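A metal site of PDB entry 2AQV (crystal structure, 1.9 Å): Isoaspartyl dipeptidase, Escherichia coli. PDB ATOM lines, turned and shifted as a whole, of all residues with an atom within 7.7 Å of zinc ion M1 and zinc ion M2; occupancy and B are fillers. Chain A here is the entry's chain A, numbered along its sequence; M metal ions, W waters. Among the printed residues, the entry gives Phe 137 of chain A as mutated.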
ATOM      1  N   HIS A  68      26.071   0.923  28.227  1.00  0.00           N
ATOM      2  CA  HIS A  68      25.885   1.177  26.821  1.00  0.00           C
ATOM      3  C   HIS A  68      24.993   2.386  26.583  1.00  0.00           C
ATOM      4  O   HIS A  68      23.798   2.255  26.308  1.00  0.00           O
ATOM      5  CB  HIS A  68      25.255  -0.082  26.165  1.00  0.00           C
ATOM      6  CG  HIS A  68      25.317  -0.016  24.669  1.00  0.00           C
ATOM      7  ND1 HIS A  68      26.034  -0.953  23.976  1.00  0.00           N
ATOM      8  CD2 HIS A  68      24.791   0.877  23.764  1.00  0.00           C
ATOM      9  CE1 HIS A  68      25.945  -0.662  22.688  1.00  0.00           C
ATOM     10  NE2 HIS A  68      25.207   0.433  22.541  1.00  0.00           N
ATOM     11  N   VAL A  69      25.585   3.572  26.696  1.00  0.00           N
ATOM     12  CA  VAL A  69      24.869   4.844  26.518  1.00  0.00           C
ATOM     13  C   VAL A  69      25.602   5.754  25.550  1.00  0.00           C
ATOM     14  O   VAL A  69      26.833   5.944  25.647  1.00  0.00           O
ATOM     15  CB  VAL A  69      24.828   5.668  27.827  1.00  0.00           C
ATOM     16  CG1 VAL A  69      23.891   6.872  27.636  1.00  0.00           C
ATOM     17  CG2 VAL A  69      24.250   4.822  28.962  1.00  0.00           C
ATOM     18  N   HIS A  70      24.829   6.351  24.661  1.00  0.00           N
ATOM     19  CA  HIS A  70      25.336   7.317  23.704  1.00  0.00           C
ATOM     20  C   HIS A  70      25.278   8.709  24.315  1.00  0.00           C
ATOM     21  O   HIS A  70      24.442   9.561  23.948  1.00  0.00           O
ATOM     22  CB  HIS A  70      24.496   7.285  22.433  1.00  0.00           C
ATOM     23  CG  HIS A  70      24.705   5.942  21.822  1.00  0.00           C
ATOM     24  ND1 HIS A  70      25.707   5.708  20.880  1.00  0.00           N
ATOM     25  CD2 HIS A  70      24.040   4.774  22.073  1.00  0.00           C
ATOM     26  CE1 HIS A  70      25.654   4.416  20.592  1.00  0.00           C
ATOM     27  NE2 HIS A  70      24.646   3.858  21.265  1.00  0.00           N
ATOM     28  N   LEU A 103      29.704   5.480  24.613  1.00  0.00           N
ATOM     29  CA  LEU A 103      30.335   4.911  23.429  1.00  0.00           C
ATOM     30  C   LEU A 103      29.700   5.579  22.217  1.00  0.00           C
ATOM     31  O   LEU A 103      28.709   6.297  22.338  1.00  0.00           O
ATOM     32  CB  LEU A 103      30.150   3.367  23.253  1.00  0.00           C
ATOM     33  CG  LEU A 103      28.824   2.809  23.806  1.00  0.00           C
ATOM     34  CD1 LEU A 103      27.651   3.313  23.004  1.00  0.00           C
ATOM     35  CD2 LEU A 103      28.844   1.306  23.712  1.00  0.00           C
ATOM     36  N   LEU A 104      30.304   5.310  21.065  1.00  0.00           N
ATOM     37  CA  LEU A 104      29.833   5.836  19.762  1.00  0.00           C
ATOM     38  C   LEU A 104      29.275   4.646  18.997  1.00  0.00           C
ATOM     39  O   LEU A 104      29.501   3.480  19.384  1.00  0.00           O
ATOM     40  CB  LEU A 104      30.940   6.543  18.950  1.00  0.00           C
ATOM     41  CG  LEU A 104      31.701   7.644  19.691  1.00  0.00           C
ATOM     42  CD1 LEU A 104      32.819   8.151  18.787  1.00  0.00           C
ATOM     43  CD2 LEU A 104      30.722   8.775  20.056  1.00  0.00           C
ATOM     44  N   GLY A 105      28.518   4.987  17.953  1.00  0.00           N
ATOM     45  CA  GLY A 105      27.853   4.013  17.090  1.00  0.00           C
ATOM     46  C   GLY A 105      28.285   4.129  15.636  1.00  0.00           C
ATOM     47  O   GLY A 105      29.464   4.186  15.262  1.00  0.00           O
ATOM     48  N   THR A 106      27.256   4.107  14.804  1.00  0.00           N
ATOM     49  CA  THR A 106      27.377   4.200  13.356  1.00  0.00           C
ATOM     50  C   THR A 106      28.250   5.378  12.905  1.00  0.00           C
ATOM     51  O   THR A 106      29.216   5.205  12.185  1.00  0.00           O
ATOM     52  CB  THR A 106      26.009   4.274  12.651  1.00  0.00           C
ATOM     53  OG1 THR A 106      25.250   3.149  13.015  1.00  0.00           O
ATOM     54  CG2 THR A 106      26.224   4.178  11.143  1.00  0.00           C
ATOM     55  N   PHE A 137      31.532   2.115  15.397  1.00  0.00           N
ATOM     56  CA  PHE A 137      31.301   0.985  14.486  1.00  0.00           C
ATOM     57  C   PHE A 137      32.522   0.663  13.611  1.00  0.00           C
ATOM     58  O   PHE A 137      32.817  -0.497  13.353  1.00  0.00           O
ATOM     59  CB  PHE A 137      30.084   1.140  13.571  1.00  0.00           C
ATOM     60  CG  PHE A 137      28.716   0.808  14.184  1.00  0.00           C
ATOM     61  CD1 PHE A 137      28.543   0.835  15.569  1.00  0.00           C
ATOM     62  CD2 PHE A 137      27.609   0.491  13.366  1.00  0.00           C
ATOM     63  CE1 PHE A 137      27.314   0.559  16.164  1.00  0.00           C
ATOM     64  CE2 PHE A 137      26.371   0.199  13.938  1.00  0.00           C
ATOM     65  CZ  PHE A 137      26.234   0.236  15.331  1.00  0.00           C
ATOM     66  N   KCX A 162      35.093  -0.151  21.133  1.00  0.00           N
ATOM     67  CA  KCX A 162      33.867  -0.594  20.543  1.00  0.00           C
ATOM     68  CB  KCX A 162      32.883   0.581  20.701  1.00  0.00           C
ATOM     69  CG  KCX A 162      31.608   0.523  19.844  1.00  0.00           C
ATOM     70  CD  KCX A 162      30.577  -0.357  20.530  1.00  0.00           C
ATOM     71  CE  KCX A 162      29.295  -0.532  19.753  1.00  0.00           C
ATOM     72  NZ  KCX A 162      28.663   0.781  19.624  1.00  0.00           N
ATOM     73  C   KCX A 162      34.082  -0.892  19.047  1.00  0.00           C
ATOM     74  O   KCX A 162      34.987  -0.338  18.396  1.00  0.00           O
ATOM     75  CX  KCX A 162      27.258   0.466  19.793  1.00  0.00           C
ATOM     76  OQ1 KCX A 162      26.845  -0.670  19.882  1.00  0.00           O
ATOM     77  OQ2 KCX A 162      26.520   1.552  19.767  1.00  0.00           O
ATOM     78  N   CYS A 163      33.214  -1.745  18.492  1.00  0.00           N
ATOM     79  CA  CYS A 163      33.157  -2.107  17.051  1.00  0.00           C
ATOM     80  C   CYS A 163      31.767  -2.680  16.673  1.00  0.00           C
ATOM     81  O   CYS A 163      30.938  -2.909  17.532  1.00  0.00           O
ATOM     82  CB  CYS A 163      34.248  -3.094  16.565  1.00  0.00           C
ATOM     83  SG  CYS A 163      33.940  -4.778  17.119  1.00  0.00           S
ATOM     84  N   ALA A 164      31.536  -2.923  15.361  1.00  0.00           N
ATOM     85  CA  ALA A 164      30.317  -3.517  14.915  1.00  0.00           C
ATOM     86  C   ALA A 164      30.669  -4.639  13.958  1.00  0.00           C
ATOM     87  O   ALA A 164      31.605  -4.514  13.147  1.00  0.00           O
ATOM     88  CB  ALA A 164      29.387  -2.543  14.153  1.00  0.00           C
ATOM     89  N   ASP A 167      26.457  -6.724  10.631  1.00  0.00           N
ATOM     90  CA  ASP A 167      25.481  -5.693  10.544  1.00  0.00           C
ATOM     91  C   ASP A 167      25.751  -4.941   9.258  1.00  0.00           C
ATOM     92  O   ASP A 167      26.902  -4.732   8.845  1.00  0.00           O
ATOM     93  CB  ASP A 167      25.689  -4.739  11.753  1.00  0.00           C
ATOM     94  CG  ASP A 167      24.639  -3.653  11.861  1.00  0.00           C
ATOM     95  OD1 ASP A 167      24.543  -2.711  11.093  1.00  0.00           O
ATOM     96  OD2 ASP A 167      23.826  -3.844  12.859  1.00  0.00           O
ATOM     97  N   ARG A 169      25.687  -2.011   8.763  1.00  0.00           N
ATOM     98  CA  ARG A 169      26.340  -0.725   9.000  1.00  0.00           C
ATOM     99  C   ARG A 169      27.812  -0.928   9.379  1.00  0.00           C
ATOM    100  O   ARG A 169      28.483   0.014   9.823  1.00  0.00           O
ATOM    101  CB  ARG A 169      25.660   0.118  10.081  1.00  0.00           C
ATOM    102  CG  ARG A 169      24.349   0.700   9.601  1.00  0.00           C
ATOM    103  CD  ARG A 169      23.394   1.004  10.746  1.00  0.00           C
ATOM    104  NE  ARG A 169      23.067  -0.196  11.490  1.00  0.00           N
ATOM    105  CZ  ARG A 169      22.470  -0.260  12.668  1.00  0.00           C
ATOM    106  NH1 ARG A 169      22.088   0.830  13.345  1.00  0.00           N
ATOM    107  NH2 ARG A 169      22.254  -1.468  13.179  1.00  0.00           N
ATOM    108  N   VAL A 199      33.823  -4.633  22.807  1.00  0.00           N
ATOM    109  CA  VAL A 199      32.374  -4.703  22.773  1.00  0.00           C
ATOM    110  C   VAL A 199      31.896  -4.754  21.326  1.00  0.00           C
ATOM    111  O   VAL A 199      32.222  -3.849  20.504  1.00  0.00           O
ATOM    112  CB  VAL A 199      31.726  -3.510  23.517  1.00  0.00           C
ATOM    113  CG1 VAL A 199      30.193  -3.550  23.387  1.00  0.00           C
ATOM    114  CG2 VAL A 199      32.157  -3.416  24.988  1.00  0.00           C
ATOM    115  N   PHE A 200      31.114  -5.796  21.001  1.00  0.00           N
ATOM    116  CA  PHE A 200      30.667  -5.902  19.632  1.00  0.00           C
ATOM    117  C   PHE A 200      29.192  -5.623  19.454  1.00  0.00           C
ATOM    118  O   PHE A 200      28.374  -6.388  19.928  1.00  0.00           O
ATOM    119  CB  PHE A 200      30.871  -7.361  19.163  1.00  0.00           C
ATOM    120  CG  PHE A 200      32.293  -7.852  19.255  1.00  0.00           C
ATOM    121  CD1 PHE A 200      32.800  -8.303  20.475  1.00  0.00           C
ATOM    122  CD2 PHE A 200      33.098  -7.900  18.119  1.00  0.00           C
ATOM    123  CE1 PHE A 200      34.116  -8.763  20.577  1.00  0.00           C
ATOM    124  CE2 PHE A 200      34.410  -8.399  18.203  1.00  0.00           C
ATOM    125  CZ  PHE A 200      34.922  -8.800  19.433  1.00  0.00           C
ATOM    126  N   HIS A 201      28.879  -4.566  18.707  1.00  0.00           N
ATOM    127  CA  HIS A 201      27.493  -4.269  18.366  1.00  0.00           C
ATOM    128  C   HIS A 201      27.109  -5.389  17.416  1.00  0.00           C
ATOM    129  O   HIS A 201      27.764  -5.554  16.380  1.00  0.00           O
ATOM    130  CB  HIS A 201      27.316  -2.918  17.577  1.00  0.00           C
ATOM    131  CG  HIS A 201      26.108  -2.895  16.675  1.00  0.00           C
ATOM    132  ND1 HIS A 201      24.962  -2.195  17.009  1.00  0.00           N
ATOM    133  CD2 HIS A 201      25.858  -3.479  15.484  1.00  0.00           C
ATOM    134  CE1 HIS A 201      24.059  -2.317  16.037  1.00  0.00           C
ATOM    135  NE2 HIS A 201      24.563  -3.098  15.106  1.00  0.00           N
ATOM    136  N   MET A 202      26.073  -6.145  17.726  1.00  0.00           N
ATOM    137  CA  MET A 202      25.688  -7.203  16.789  1.00  0.00           C
ATOM    138  C   MET A 202      24.516  -6.732  15.929  1.00  0.00           C
ATOM    139  O   MET A 202      23.584  -6.103  16.436  1.00  0.00           O
ATOM    140  CB  MET A 202      25.179  -8.455  17.546  1.00  0.00           C
ATOM    141  CG  MET A 202      26.180  -9.126  18.462  1.00  0.00           C
ATOM    142  SD  MET A 202      27.782  -9.444  17.699  1.00  0.00           S
ATOM    143  CE  MET A 202      27.266 -10.618  16.407  1.00  0.00           C
ATOM    144  N   GLY A 203      24.512  -7.049  14.644  1.00  0.00           N
ATOM    145  CA  GLY A 203      23.391  -6.684  13.818  1.00  0.00           C
ATOM    146  C   GLY A 203      22.631  -7.971  13.462  1.00  0.00           C
ATOM    147  O   GLY A 203      22.778  -8.997  14.124  1.00  0.00           O
ATOM    148  N   THR A 229      26.873  -7.523  22.292  1.00  0.00           N
ATOM    149  CA  THR A 229      25.739  -6.778  22.787  1.00  0.00           C
ATOM    150  C   THR A 229      24.548  -6.833  21.816  1.00  0.00           C
ATOM    151  O   THR A 229      24.757  -7.250  20.688  1.00  0.00           O
ATOM    152  CB  THR A 229      26.128  -5.381  23.308  1.00  0.00           C
ATOM    153  OG1 THR A 229      24.971  -4.866  23.905  1.00  0.00           O
ATOM    154  CG2 THR A 229      26.562  -4.479  22.162  1.00  0.00           C
ATOM    155  N   HIS A 230      23.308  -6.513  22.263  1.00  0.00           N
ATOM    156  CA  HIS A 230      22.082  -6.584  21.458  1.00  0.00           C
ATOM    157  C   HIS A 230      21.771  -8.044  21.058  1.00  0.00           C
ATOM    158  O   HIS A 230      21.190  -8.285  20.010  1.00  0.00           O
ATOM    159  CB  HIS A 230      22.149  -5.773  20.128  1.00  0.00           C
ATOM    160  CG  HIS A 230      22.776  -4.431  20.256  1.00  0.00           C
ATOM    161  ND1 HIS A 230      22.411  -3.560  21.289  1.00  0.00           N
ATOM    162  CD2 HIS A 230      23.739  -3.840  19.523  1.00  0.00           C
ATOM    163  CE1 HIS A 230      23.133  -2.461  21.161  1.00  0.00           C
ATOM    164  NE2 HIS A 230      23.940  -2.611  20.129  1.00  0.00           N
ATOM    165  N   ARG A 233      18.249  -9.377  19.832  1.00  0.00           N
ATOM    166  CA  ARG A 233      17.715  -8.776  18.583  1.00  0.00           C
ATOM    167  C   ARG A 233      17.111  -9.734  17.571  1.00  0.00           C
ATOM    168  O   ARG A 233      16.258  -9.357  16.753  1.00  0.00           O
ATOM    169  CB  ARG A 233      18.672  -7.821  17.902  1.00  0.00           C
ATOM    170  CG  ARG A 233      19.945  -8.524  17.406  1.00  0.00           C
ATOM    171  CD  ARG A 233      20.875  -7.597  16.620  1.00  0.00           C
ATOM    172  NE  ARG A 233      20.096  -6.681  15.795  1.00  0.00           N
ATOM    173  CZ  ARG A 233      20.158  -5.345  15.783  1.00  0.00           C
ATOM    174  NH1 ARG A 233      20.984  -4.596  16.549  1.00  0.00           N
ATOM    175  NH2 ARG A 233      19.329  -4.732  14.967  1.00  0.00           N
ATOM    176  N   THR A 254      20.006  -6.040  25.577  1.00  0.00           N
ATOM    177  CA  THR A 254      19.610  -4.655  25.472  1.00  0.00           C
ATOM    178  C   THR A 254      18.171  -4.473  25.907  1.00  0.00           C
ATOM    179  O   THR A 254      17.275  -5.116  25.346  1.00  0.00           O
ATOM    180  CB  THR A 254      19.827  -4.107  24.039  1.00  0.00           C
ATOM    181  OG1 THR A 254      21.157  -4.412  23.655  1.00  0.00           O
ATOM    182  CG2 THR A 254      19.556  -2.598  23.910  1.00  0.00           C
ATOM    183  N   SER A 284      21.209  -0.293  28.273  1.00  0.00           N
ATOM    184  CA  SER A 284      20.113   0.342  27.631  1.00  0.00           C
ATOM    185  C   SER A 284      20.221   0.706  26.167  1.00  0.00           C
ATOM    186  O   SER A 284      19.177   0.721  25.478  1.00  0.00           O
ATOM    187  CB  SER A 284      19.649   1.600  28.414  1.00  0.00           C
ATOM    188  OG  SER A 284      20.649   2.608  28.324  1.00  0.00           O
ATOM    189  N   ASP A 285      21.419   1.076  25.718  1.00  0.00           N
ATOM    190  CA  ASP A 285      21.585   1.634  24.387  1.00  0.00           C
ATOM    191  C   ASP A 285      20.867   3.006  24.384  1.00  0.00           C
ATOM    192  O   ASP A 285      20.418   3.536  23.356  1.00  0.00           O
ATOM    193  CB  ASP A 285      21.078   0.743  23.231  1.00  0.00           C
ATOM    194  CG  ASP A 285      21.797   1.135  21.947  1.00  0.00           C
ATOM    195  OD1 ASP A 285      22.631   1.994  21.921  1.00  0.00           O
ATOM    196  OD2 ASP A 285      21.431   0.518  20.857  1.00  0.00           O
ATOM    197  N   GLY A 286      20.740   3.586  25.594  1.00  0.00           N
ATOM    198  CA  GLY A 286      20.066   4.873  25.784  1.00  0.00           C
ATOM    199  C   GLY A 286      20.672   6.003  24.938  1.00  0.00           C
ATOM    200  O   GLY A 286      21.900   6.142  24.759  1.00  0.00           O
ATOM    201  N   ASN A 287      19.760   6.827  24.432  1.00  0.00           N
ATOM    202  CA  ASN A 287      20.093   7.967  23.583  1.00  0.00           C
ATOM    203  C   ASN A 287      20.486   7.626  22.147  1.00  0.00           C
ATOM    204  O   ASN A 287      20.943   8.490  21.402  1.00  0.00           O
ATOM    205  CB  ASN A 287      21.032   8.988  24.212  1.00  0.00           C
ATOM    206  CG  ASN A 287      20.325  10.305  24.403  1.00  0.00           C
ATOM    207  OD1 ASN A 287      19.135  10.341  24.745  1.00  0.00           O
ATOM    208  ND2 ASN A 287      21.111  11.359  24.175  1.00  0.00           N
ATOM    209  N   GLY A 288      20.292   6.350  21.758  1.00  0.00           N
ATOM    210  CA  GLY A 288      20.604   5.883  20.410  1.00  0.00           C
ATOM    211  C   GLY A 288      19.458   6.125  19.410  1.00  0.00           C
ATOM    212  O   GLY A 288      18.515   6.879  19.675  1.00  0.00           O
HETATM  213 ZN    ZN M   1      24.731  -1.071  18.937  1.00  0.00          ZN
HETATM  214 ZN    ZN M   2      24.571   1.661  20.792  1.00  0.00          ZN
HETATM  215  O   HOH W   1      23.383   1.116  18.542  1.00  0.00           O
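A ring nitrogen (ND1) of His 230 is in hydrogen-bond range of the side-chain hydroxyl (OG1) of Thr 254 (2.8 Å). The backbone NH (N) of His 201 sits at hydrogen-bond distance from the backbone carbonyl oxygen (O) of Cys 163 (2.9 Å). A ring nitrogen (NE2) of His 201 sits at hydrogen-bond distance from the guanidinium group (NH2) of Arg 169. O of His 68 sits at hydrogen-bond distance from N of Gly 286 (3.4 Å). N of His 70 lies within hydrogen-bond range of O of Gly 286 (2.9 Å). A ring nitrogen (NE2) of His 201 is in hydrogen-bond range of the side-chain carboxylate (OD2) of Asp 167 (2.5 Å). O of Leu 103 lies within hydrogen-bond range of ND1 of His 70 (3.4 Å). NZ of KCX 162 is in hydrogen-bond range of the backbone carbonyl oxygen of Leu 104.
The nearest printed residue that does not touch zinc ion M1 is Phe 137 (4.1 Å).
A ring nitrogen (NE2) of His 230 is bound to zinc ion M1 (2.1 Å). ND1 of His 201 binds zinc ion M1 (2.2 Å). Zinc ion M1 is bound by OQ1 of KCX 162 (2.4 Å). Water W1 binds zinc ion M1 (2.6 Å).
Zinc ion M2 is bound by OQ2 of KCX 162, NE2 of His 68, NE2 of His 70 and OD1 of Asp 285. Zinc ion M2 has four donor atoms within binding distance. Slightly farther from zinc ion M2 lies water W1 (2.6 Å).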
